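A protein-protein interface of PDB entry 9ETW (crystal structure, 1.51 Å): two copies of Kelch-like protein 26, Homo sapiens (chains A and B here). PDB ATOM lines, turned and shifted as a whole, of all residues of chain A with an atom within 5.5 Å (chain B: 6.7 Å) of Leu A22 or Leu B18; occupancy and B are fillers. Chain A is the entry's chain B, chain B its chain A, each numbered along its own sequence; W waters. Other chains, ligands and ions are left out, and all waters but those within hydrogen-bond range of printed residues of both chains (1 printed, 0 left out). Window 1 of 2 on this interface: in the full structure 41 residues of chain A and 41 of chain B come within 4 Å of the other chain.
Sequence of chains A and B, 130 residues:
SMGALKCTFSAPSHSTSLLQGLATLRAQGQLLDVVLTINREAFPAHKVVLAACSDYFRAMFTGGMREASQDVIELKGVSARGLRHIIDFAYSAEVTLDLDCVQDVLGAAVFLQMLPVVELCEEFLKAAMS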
ATOM      1  N   SER A  17     -21.747  14.109 -13.834  1.00  0.00           N
ATOM      2  CA  SER A  17     -21.846  15.205 -12.874  1.00  0.00           C
ATOM      3  C   SER A  17     -21.457  14.752 -11.486  1.00  0.00           C
ATOM      4  O   SER A  17     -20.825  15.504 -10.734  1.00  0.00           O
ATOM      5  CB  SER A  17     -23.263  15.749 -12.857  1.00  0.00           C
ATOM      6  OG  SER A  17     -23.537  16.343 -14.113  1.00  0.00           O
ATOM      7  N   LEU A  18     -21.849  13.530 -11.131  1.00  0.00           N
ATOM      8  CA  LEU A  18     -21.501  12.972  -9.830  1.00  0.00           C
ATOM      9  C   LEU A  18     -19.995  12.836  -9.716  1.00  0.00           C
ATOM     10  O   LEU A  18     -19.396  13.237  -8.709  1.00  0.00           O
ATOM     11  CB  LEU A  18     -22.200  11.615  -9.652  1.00  0.00           C
ATOM     12  CG  LEU A  18     -21.984  10.925  -8.305  1.00  0.00           C
ATOM     13  CD1 LEU A  18     -22.765  11.633  -7.261  1.00  0.00           C
ATOM     14  CD2 LEU A  18     -22.441   9.471  -8.363  1.00  0.00           C
ATOM     15  N   LEU A  19     -19.363  12.297 -10.760  1.00  0.00           N
ATOM     16  CA  LEU A  19     -17.902  12.161 -10.746  1.00  0.00           C
ATOM     17  C   LEU A  19     -17.230  13.525 -10.555  1.00  0.00           C
ATOM     18  O   LEU A  19     -16.315  13.680  -9.739  1.00  0.00           O
ATOM     19  CB  LEU A  19     -17.429  11.478 -12.034  1.00  0.00           C
ATOM     20  CG  LEU A  19     -15.926  11.292 -12.243  1.00  0.00           C
ATOM     21  CD1 LEU A  19     -15.410  10.371 -11.162  1.00  0.00           C
ATOM     22  CD2 LEU A  19     -15.597  10.719 -13.631  1.00  0.00           C
ATOM     23  N   GLN A  20     -17.685  14.543 -11.283  1.00  0.00           N
ATOM     24  CA  GLN A  20     -17.108  15.877 -11.121  1.00  0.00           C
ATOM     25  C   GLN A  20     -17.295  16.373  -9.694  1.00  0.00           C
ATOM     26  O   GLN A  20     -16.402  17.011  -9.123  1.00  0.00           O
ATOM     27  CB  GLN A  20     -17.738  16.856 -12.129  1.00  0.00           C
ATOM     28  CG  GLN A  20     -17.181  18.291 -12.053  1.00  0.00           C
ATOM     29  CD  GLN A  20     -17.720  19.250 -13.140  1.00  0.00           C
ATOM     30  OE1 GLN A  20     -18.863  19.133 -13.595  1.00  0.00           O
ATOM     31  NE2 GLN A  20     -16.892  20.217 -13.537  1.00  0.00           N
ATOM     32  N   GLY A  21     -18.448  16.069  -9.088  1.00  0.00           N
ATOM     33  CA  GLY A  21     -18.686  16.505  -7.725  1.00  0.00           C
ATOM     34  C   GLY A  21     -17.784  15.803  -6.736  1.00  0.00           C
ATOM     35  O   GLY A  21     -17.270  16.420  -5.805  1.00  0.00           O
ATOM     36  N   LEU A  22     -17.521  14.521  -6.963  1.00  0.00           N
ATOM     37  CA  LEU A  22     -16.597  13.808  -6.093  1.00  0.00           C
ATOM     38  C   LEU A  22     -15.216  14.442  -6.158  1.00  0.00           C
ATOM     39  O   LEU A  22     -14.548  14.610  -5.124  1.00  0.00           O
ATOM     40  CB  LEU A  22     -16.537  12.333  -6.495  1.00  0.00           C
ATOM     41  CG  LEU A  22     -17.857  11.594  -6.303  1.00  0.00           C
ATOM     42  CD1 LEU A  22     -17.767  10.237  -7.016  1.00  0.00           C
ATOM     43  CD2 LEU A  22     -18.119  11.418  -4.809  1.00  0.00           C
ATOM     44  N   ALA A  23     -14.767  14.797  -7.372  1.00  0.00           N
ATOM     45  CA  ALA A  23     -13.438  15.379  -7.523  1.00  0.00           C
ATOM     46  C   ALA A  23     -13.366  16.756  -6.854  1.00  0.00           C
ATOM     47  O   ALA A  23     -12.349  17.094  -6.232  1.00  0.00           O
ATOM     48  CB  ALA A  23     -13.057  15.466  -9.008  1.00  0.00           C
ATOM     49  N   THR A  24     -14.442  17.552  -6.930  1.00  0.00           N
ATOM     50  CA  THR A  24     -14.368  18.876  -6.281  1.00  0.00           C
ATOM     51  C   THR A  24     -14.370  18.715  -4.764  1.00  0.00           C
ATOM     52  O   THR A  24     -13.717  19.505  -4.053  1.00  0.00           O
ATOM     53  CB  THR A  24     -15.503  19.809  -6.719  1.00  0.00           C
ATOM     54  OG1 THR A  24     -16.759  19.338  -6.193  1.00  0.00           O
ATOM     55  CG2 THR A  24     -15.550  19.933  -8.249  1.00  0.00           C
ATOM     56  N   LEU A  25     -15.052  17.679  -4.259  1.00  0.00           N
ATOM     57  CA  LEU A  25     -15.019  17.428  -2.823  1.00  0.00           C
ATOM     58  C   LEU A  25     -13.629  16.989  -2.374  1.00  0.00           C
ATOM     59  O   LEU A  25     -13.134  17.435  -1.335  1.00  0.00           O
ATOM     60  CB  LEU A  25     -16.073  16.380  -2.423  1.00  0.00           C
ATOM     61  CG  LEU A  25     -17.507  16.928  -2.443  1.00  0.00           C
ATOM     62  CD1 LEU A  25     -18.535  15.808  -2.626  1.00  0.00           C
ATOM     63  CD2 LEU A  25     -17.805  17.737  -1.149  1.00  0.00           C
ATOM     64  N   ARG A  26     -12.974  16.106  -3.122  1.00  0.00           N
ATOM     65  CA  ARG A  26     -11.609  15.751  -2.734  1.00  0.00           C
ATOM     66  C   ARG A  26     -10.700  16.985  -2.744  1.00  0.00           C
ATOM     67  O   ARG A  26      -9.902  17.203  -1.817  1.00  0.00           O
ATOM     68  CB  ARG A  26     -11.068  14.658  -3.664  1.00  0.00           C
ATOM     69  CG  ARG A  26      -9.677  14.189  -3.233  1.00  0.00           C
ATOM     70  CD  ARG A  26      -9.064  13.196  -4.205  1.00  0.00           C
ATOM     71  NE  ARG A  26      -7.833  12.674  -3.633  1.00  0.00           N
ATOM     72  CZ  ARG A  26      -6.677  12.585  -4.282  1.00  0.00           C
ATOM     73  NH1 ARG A  26      -6.581  12.944  -5.559  1.00  0.00           N
ATOM     74  NH2 ARG A  26      -5.601  12.085  -3.645  1.00  0.00           N
ATOM     75  N   ALA A  27     -10.810  17.809  -3.790  1.00  0.00           N
ATOM     76  CA  ALA A  27      -9.940  18.974  -3.931  1.00  0.00           C
ATOM     77  C   ALA A  27     -10.169  19.986  -2.817  1.00  0.00           C
ATOM     78  O   ALA A  27      -9.242  20.703  -2.418  1.00  0.00           O
ATOM     79  CB  ALA A  27     -10.162  19.625  -5.303  1.00  0.00           C
ATOM     80  N   HIS A  46     -11.570   9.145  -0.572  1.00  0.00           N
ATOM     81  CA  HIS A  46     -12.817   8.611  -0.032  1.00  0.00           C
ATOM     82  C   HIS A  46     -12.830   7.107  -0.242  1.00  0.00           C
ATOM     83  O   HIS A  46     -12.777   6.637  -1.387  1.00  0.00           O
ATOM     84  CB  HIS A  46     -14.007   9.227  -0.753  1.00  0.00           C
ATOM     85  CG  HIS A  46     -14.058  10.714  -0.647  1.00  0.00           C
ATOM     86  ND1 HIS A  46     -13.611  11.552  -1.650  1.00  0.00           N
ATOM     87  CD2 HIS A  46     -14.490  11.523   0.358  1.00  0.00           C
ATOM     88  CE1 HIS A  46     -13.775  12.808  -1.273  1.00  0.00           C
ATOM     89  NE2 HIS A  46     -14.310  12.817  -0.060  1.00  0.00           N
ATOM     90  N   VAL A  49     -15.260   5.762  -2.876  1.00  0.00           N
ATOM     91  CA  VAL A  49     -14.944   6.021  -4.273  1.00  0.00           C
ATOM     92  C   VAL A  49     -13.914   5.022  -4.789  1.00  0.00           C
ATOM     93  O   VAL A  49     -14.059   4.468  -5.882  1.00  0.00           O
ATOM     94  CB  VAL A  49     -14.447   7.470  -4.442  1.00  0.00           C
ATOM     95  CG1 VAL A  49     -13.914   7.669  -5.829  1.00  0.00           C
ATOM     96  CG2 VAL A  49     -15.562   8.420  -4.167  1.00  0.00           C
ATOM     97  N   ALA A  52     -15.390   1.604  -5.169  1.00  0.00           N
ATOM     98  CA  ALA A  52     -16.371   1.483  -6.237  1.00  0.00           C
ATOM     99  C   ALA A  52     -15.742   1.255  -7.603  1.00  0.00           C
ATOM    100  O   ALA A  52     -16.480   0.968  -8.549  1.00  0.00           O
ATOM    101  CB  ALA A  52     -17.250   2.739  -6.302  1.00  0.00           C
ATOM    102  N   CYS A  53     -14.422   1.429  -7.750  1.00  0.00           N
ATOM    103  CA  CYS A  53     -13.811   1.202  -9.058  1.00  0.00           C
ATOM    104  C   CYS A  53     -12.582   0.295  -9.022  1.00  0.00           C
ATOM    105  O   CYS A  53     -11.927   0.132 -10.057  1.00  0.00           O
ATOM    106  CB  CYS A  53     -13.462   2.532  -9.744  1.00  0.00           C
ATOM    107  SG  CYS A  53     -12.286   3.574  -8.887  1.00  0.00           S
ATOM    108  N   ALA A  90      -9.417   7.619 -10.634  1.00  0.00           N
ATOM    109  CA  ALA A  90     -10.693   7.275  -9.997  1.00  0.00           C
ATOM    110  C   ALA A  90     -11.639   8.476  -9.956  1.00  0.00           C
ATOM    111  O   ALA A  90     -12.857   8.323 -10.122  1.00  0.00           O
ATOM    112  CB  ALA A  90     -10.435   6.761  -8.583  1.00  0.00           C
ATOM    113  N   TYR A  91     -11.091   9.672  -9.734  1.00  0.00           N
ATOM    114  CA  TYR A  91     -11.877  10.890  -9.604  1.00  0.00           C
ATOM    115  C   TYR A  91     -12.057  11.671 -10.912  1.00  0.00           C
ATOM    116  O   TYR A  91     -12.740  12.705 -10.910  1.00  0.00           O
ATOM    117  CB  TYR A  91     -11.216  11.798  -8.568  1.00  0.00           C
ATOM    118  CG  TYR A  91     -11.391  11.347  -7.139  1.00  0.00           C
ATOM    119  CD1 TYR A  91     -10.507  10.444  -6.553  1.00  0.00           C
ATOM    120  CD2 TYR A  91     -12.483  11.799  -6.377  1.00  0.00           C
ATOM    121  CE1 TYR A  91     -10.685  10.029  -5.250  1.00  0.00           C
ATOM    122  CE2 TYR A  91     -12.662  11.387  -5.079  1.00  0.00           C
ATOM    123  CZ  TYR A  91     -11.762  10.504  -4.518  1.00  0.00           C
ATOM    124  OH  TYR A  91     -11.939  10.129  -3.211  1.00  0.00           O
ATOM    125  N   SER B  13     -16.390   4.902 -20.101  1.00  0.00           N
ATOM    126  CA  SER B  13     -17.234   4.042 -19.283  1.00  0.00           C
ATOM    127  C   SER B  13     -17.010   4.215 -17.780  1.00  0.00           C
ATOM    128  O   SER B  13     -17.736   3.594 -16.992  1.00  0.00           O
ATOM    129  CB  SER B  13     -16.981   2.574 -19.655  1.00  0.00           C
ATOM    130  OG  SER B  13     -15.680   2.180 -19.200  1.00  0.00           O
ATOM    131  N   HIS B  14     -16.020   5.017 -17.358  1.00  0.00           N
ATOM    132  CA  HIS B  14     -15.619   4.967 -15.948  1.00  0.00           C
ATOM    133  C   HIS B  14     -16.692   5.532 -15.031  1.00  0.00           C
ATOM    134  O   HIS B  14     -16.962   4.957 -13.972  1.00  0.00           O
ATOM    135  CB  HIS B  14     -14.283   5.683 -15.727  1.00  0.00           C
ATOM    136  CG  HIS B  14     -13.925   5.870 -14.281  1.00  0.00           C
ATOM    137  ND1 HIS B  14     -13.568   4.831 -13.452  1.00  0.00           N
ATOM    138  CD2 HIS B  14     -13.908   6.994 -13.512  1.00  0.00           C
ATOM    139  CE1 HIS B  14     -13.314   5.307 -12.238  1.00  0.00           C
ATOM    140  NE2 HIS B  14     -13.516   6.615 -12.250  1.00  0.00           N
ATOM    141  N   SER B  15     -17.307   6.658 -15.397  1.00  0.00           N
ATOM    142  CA  SER B  15     -18.267   7.260 -14.478  1.00  0.00           C
ATOM    143  C   SER B  15     -19.472   6.348 -14.292  1.00  0.00           C
ATOM    144  O   SER B  15     -20.044   6.282 -13.200  1.00  0.00           O
ATOM    145  CB  SER B  15     -18.694   8.645 -14.963  1.00  0.00           C
ATOM    146  OG  SER B  15     -19.483   8.578 -16.148  1.00  0.00           O
ATOM    147  N   THR B  16     -19.861   5.620 -15.349  1.00  0.00           N
ATOM    148  CA  THR B  16     -20.974   4.674 -15.240  1.00  0.00           C
ATOM    149  C   THR B  16     -20.602   3.477 -14.371  1.00  0.00           C
ATOM    150  O   THR B  16     -21.396   3.030 -13.538  1.00  0.00           O
ATOM    151  CB  THR B  16     -21.391   4.199 -16.637  1.00  0.00           C
ATOM    152  OG1 THR B  16     -21.859   5.324 -17.383  1.00  0.00           O
ATOM    153  CG2 THR B  16     -22.514   3.160 -16.541  1.00  0.00           C
ATOM    154  N   SER B  17     -19.407   2.927 -14.567  1.00  0.00           N
ATOM    155  CA  SER B  17     -18.969   1.816 -13.730  1.00  0.00           C
ATOM    156  C   SER B  17     -18.841   2.235 -12.269  1.00  0.00           C
ATOM    157  O   SER B  17     -19.142   1.448 -11.356  1.00  0.00           O
ATOM    158  CB  SER B  17     -17.625   1.296 -14.243  1.00  0.00           C
ATOM    159  OG  SER B  17     -17.729   0.846 -15.576  1.00  0.00           O
ATOM    160  N   LEU B  18     -18.337   3.451 -12.032  1.00  0.00           N
ATOM    161  CA  LEU B  18     -18.201   3.958 -10.666  1.00  0.00           C
ATOM    162  C   LEU B  18     -19.560   4.085 -10.001  1.00  0.00           C
ATOM    163  O   LEU B  18     -19.751   3.667  -8.845  1.00  0.00           O
ATOM    164  CB  LEU B  18     -17.489   5.317 -10.672  1.00  0.00           C
ATOM    165  CG  LEU B  18     -17.120   5.899  -9.294  1.00  0.00           C
ATOM    166  CD1 LEU B  18     -15.885   5.161  -8.771  1.00  0.00           C
ATOM    167  CD2 LEU B  18     -16.887   7.416  -9.378  1.00  0.00           C
ATOM    168  N   LEU B  19     -20.525   4.673 -10.713  1.00  0.00           N
ATOM    169  CA  LEU B  19     -21.871   4.779 -10.154  1.00  0.00           C
ATOM    170  C   LEU B  19     -22.400   3.398  -9.764  1.00  0.00           C
ATOM    171  O   LEU B  19     -22.925   3.203  -8.661  1.00  0.00           O
ATOM    172  CB  LEU B  19     -22.799   5.464 -11.161  1.00  0.00           C
ATOM    173  CG  LEU B  19     -24.244   5.700 -10.735  1.00  0.00           C
ATOM    174  CD1 LEU B  19     -24.268   6.644  -9.539  1.00  0.00           C
ATOM    175  CD2 LEU B  19     -25.046   6.246 -11.920  1.00  0.00           C
ATOM    176  N   GLN B  20     -22.256   2.413 -10.659  1.00  0.00           N
ATOM    177  CA  GLN B  20     -22.707   1.056 -10.351  1.00  0.00           C
ATOM    178  C   GLN B  20     -22.008   0.525  -9.110  1.00  0.00           C
ATOM    179  O   GLN B  20     -22.632  -0.136  -8.265  1.00  0.00           O
ATOM    180  CB  GLN B  20     -22.457   0.116 -11.533  1.00  0.00           C
ATOM    181  CG  GLN B  20     -22.945  -1.330 -11.271  1.00  0.00           C
ATOM    182  CD  GLN B  20     -22.547  -2.324 -12.360  1.00  0.00           C
ATOM    183  OE1 GLN B  20     -21.473  -2.218 -12.963  1.00  0.00           O
ATOM    184  NE2 GLN B  20     -23.407  -3.306 -12.601  1.00  0.00           N
ATOM    185  N   GLY B  21     -20.705   0.796  -8.988  1.00  0.00           N
ATOM    186  CA  GLY B  21     -19.968   0.373  -7.803  1.00  0.00           C
ATOM    187  C   GLY B  21     -20.510   1.012  -6.535  1.00  0.00           C
ATOM    188  O   GLY B  21     -20.652   0.344  -5.507  1.00  0.00           O
ATOM    189  N   LEU B  22     -20.796   2.325  -6.575  1.00  0.00           N
ATOM    190  CA  LEU B  22     -21.394   2.975  -5.400  1.00  0.00           C
ATOM    191  C   LEU B  22     -22.713   2.317  -5.015  1.00  0.00           C
ATOM    192  O   LEU B  22     -22.988   2.089  -3.830  1.00  0.00           O
ATOM    193  CB  LEU B  22     -21.630   4.465  -5.675  1.00  0.00           C
ATOM    194  CG  LEU B  22     -20.327   5.228  -5.939  1.00  0.00           C
ATOM    195  CD1 LEU B  22     -20.657   6.605  -6.479  1.00  0.00           C
ATOM    196  CD2 LEU B  22     -19.525   5.379  -4.664  1.00  0.00           C
ATOM    197  N   ALA B  23     -23.560   2.037  -6.003  1.00  0.00           N
ATOM    198  CA  ALA B  23     -24.848   1.397  -5.730  1.00  0.00           C
ATOM    199  C   ALA B  23     -24.659   0.033  -5.066  1.00  0.00           C
ATOM    200  O   ALA B  23     -25.375  -0.300  -4.103  1.00  0.00           O
ATOM    201  CB  ALA B  23     -25.666   1.262  -7.019  1.00  0.00           C
ATOM    202  N   VAL B  48     -20.596  11.568   0.936  1.00  0.00           N
ATOM    203  CA  VAL B  48     -19.870  12.145  -0.195  1.00  0.00           C
ATOM    204  C   VAL B  48     -20.665  11.959  -1.486  1.00  0.00           C
ATOM    205  O   VAL B  48     -20.577  12.804  -2.406  1.00  0.00           O
ATOM    206  CB  VAL B  48     -18.432  11.573  -0.290  1.00  0.00           C
ATOM    207  CG1 VAL B  48     -18.398  10.124  -0.773  1.00  0.00           C
ATOM    208  CG2 VAL B  48     -17.596  12.442  -1.222  1.00  0.00           C
ATOM    209  N   VAL B  49     -21.472  10.888  -1.574  1.00  0.00           N
ATOM    210  CA  VAL B  49     -22.273  10.676  -2.776  1.00  0.00           C
ATOM    211  C   VAL B  49     -23.411  11.692  -2.843  1.00  0.00           C
ATOM    212  O   VAL B  49     -23.642  12.307  -3.886  1.00  0.00           O
ATOM    213  CB  VAL B  49     -22.805   9.236  -2.830  1.00  0.00           C
ATOM    214  CG1 VAL B  49     -23.783   9.090  -3.982  1.00  0.00           C
ATOM    215  CG2 VAL B  49     -21.648   8.252  -2.941  1.00  0.00           C
ATOM    216  N   ALA B  51     -23.495  14.585  -1.303  1.00  0.00           N
ATOM    217  CA  ALA B  51     -22.914  15.912  -1.477  1.00  0.00           C
ATOM    218  C   ALA B  51     -22.459  16.160  -2.916  1.00  0.00           C
ATOM    219  O   ALA B  51     -22.398  17.321  -3.362  1.00  0.00           O
ATOM    220  CB  ALA B  51     -21.740  16.090  -0.511  1.00  0.00           C
ATOM    221  N   ALA B  52     -22.104  15.100  -3.648  1.00  0.00           N
ATOM    222  CA  ALA B  52     -21.620  15.277  -5.007  1.00  0.00           C
ATOM    223  C   ALA B  52     -22.729  15.512  -6.011  1.00  0.00           C
ATOM    224  O   ALA B  52     -22.426  15.868  -7.154  1.00  0.00           O
ATOM    225  CB  ALA B  52     -20.772  14.071  -5.450  1.00  0.00           C
ATOM    226  N   CYS B  53     -23.999  15.360  -5.642  1.00  0.00           N
ATOM    227  CA  CYS B  53     -25.030  15.648  -6.629  1.00  0.00           C
ATOM    228  C   CYS B  53     -26.130  16.563  -6.117  1.00  0.00           C
ATOM    229  O   CYS B  53     -27.089  16.790  -6.847  1.00  0.00           O
ATOM    230  CB  CYS B  53     -25.637  14.365  -7.202  1.00  0.00           C
ATOM    231  SG  CYS B  53     -26.322  13.227  -6.016  1.00  0.00           S
ATOM    232  N   ARG B  58     -24.610  19.063   0.009  1.00  0.00           N
ATOM    233  CA  ARG B  58     -23.224  19.489   0.160  1.00  0.00           C
ATOM    234  C   ARG B  58     -23.111  20.539   1.258  1.00  0.00           C
ATOM    235  O   ARG B  58     -22.234  20.453   2.126  1.00  0.00           O
ATOM    236  CB  ARG B  58     -22.665  19.991  -1.177  1.00  0.00           C
ATOM    237  CG  ARG B  58     -21.184  20.434  -1.106  1.00  0.00           C
ATOM    238  CD  ARG B  58     -20.551  20.493  -2.490  1.00  0.00           C
ATOM    239  NE  ARG B  58     -19.123  20.818  -2.449  1.00  0.00           N
ATOM    240  CZ  ARG B  58     -18.276  20.572  -3.440  1.00  0.00           C
ATOM    241  NH1 ARG B  58     -18.668  19.947  -4.539  1.00  0.00           N
ATOM    242  NH2 ARG B  58     -17.010  20.973  -3.333  1.00  0.00           N
HETATM  243  O   HOH W   1     -23.911  15.922  -9.592  1.00  0.00           O
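The guanidinium group (NH1) of Arg B58 is in hydrogen-bond range of the side-chain hydroxyl (OG1) of Thr A24 (2.6 Å).
O of Ala A90 is in hydrogen-bond range of NE2 of His B14, 2.8 Å away.
The backbone carbonyl oxygen (O) of Ser B13 is in hydrogen-bond range of the side-chain hydroxyl (OG) of Ser B17.
O of Gly A21 lies within hydrogen-bond range of OG1 of Thr A24, at 3.0 Å.
The side-chain sulfur (SG) of Cys A53 is in hydrogen-bond range of the backbone carbonyl oxygen (O) of Val A49 (3.6 Å).
O of Val B49 sits at hydrogen-bond distance from SG of Cys B53 (3.5 Å).
A ring nitrogen (ND1) of His A46 is in hydrogen-bond range of the side-chain hydroxyl (OH) of Tyr A91.
CD1 of Leu A18 touches O of Val B49 (3.6 Å).
CD1 of Leu A19 touches CD2 of Leu B18 (3.8 Å).
Leu A22 touches Ala B52 (N to CB, 3.6 Å).
Leu A25 touches Val B48.
CB of Ala B51 touches CD1 of Leu A25, at 3.9 Å.
CD1 of Leu A25 touches N of Ala B52, at 3.8 Å.
CD2 of Leu A25 touches NE of Arg B58, at 3.6 Å.
NE2 of His A46 touches CG2 of Val B48, at 3.5 Å.
Gly B21 touches Ala A52.
Cys A53 touches Leu B18.
Printed residues of chain B within 4 Å of Leu A22: Leu B18 (3.8 Å), Val B48 (3.7 Å) and Ala B52 (3.6 Å).
Of the printed residues of chain B, Leu A25 touches Val B48, Ala B51, Ala B52 and Arg B58.
Printed residues of chain B within 4 Å of Ala A90: His B14.
Printed residues of chain A within 4 Å of Ala B51: Leu A25.
Of the printed residues of chain A, Val B49 touches Leu A18 (3.6 Å).
Ser B13 touches none of the printed residues of chain A.
The nearest printed residue of chain B that does not touch Thr A24 is Ala B52 (6.4 Å).
Printed residues of chain A that touch a printed residue of chain B: Ser A17, Leu A18, Leu A19, Gly A21, Leu A22, Thr A24, Leu A25, His A46, Val A49, Ala A52, Cys A53 and Ala A90.
Hydrophobic or aromatic side chains of chain A within 4 Å of the printed part of chain B: Leu A18, Leu A19, Leu A22, Leu A25, His A46 and Ala A52.
Of the 17 printed residues of chain B, 13 touch a printed residue of chain A.
Printed residues of chain B that touch a printed residue of chain A: His B14, Ser B15, Ser B17, Leu B18, Leu B19, Gly B21, Leu B22, Val B48, Val B49, Ala B51, Ala B52, Cys B53 and Arg B58.
Hydrophobic or aromatic side chains of chain B that line the printed part of chain A: His B14, Leu B18, Leu B19, Leu B22, Val B48, Ala B51 and Ala B52.
Among the printed residues, no Asp or Glu carboxylate lies within 4 Å of a Lys or Arg side-chain nitrogen of the other chain.
Leu A18 touches Leu B22, and with the chains exchanged Leu A22 touches Leu B18.
Leu A18 touches Val B49, and with the chains exchanged Val A49 touches Leu B18.
Gly A21 touches Ala B52, and with the chains exchanged Ala A52 touches Gly B21.
Leu A22 touches Ala B52, and with the chains exchanged Ala A52 touches Leu B22.
10 positions are printed for both chains.
Of the 27 pairs that touch across the chains among the printed residues, 16 have their exchanged pair printed and touching as well.
Water W1 bridges O of Ala B52 and O of Ser A17.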
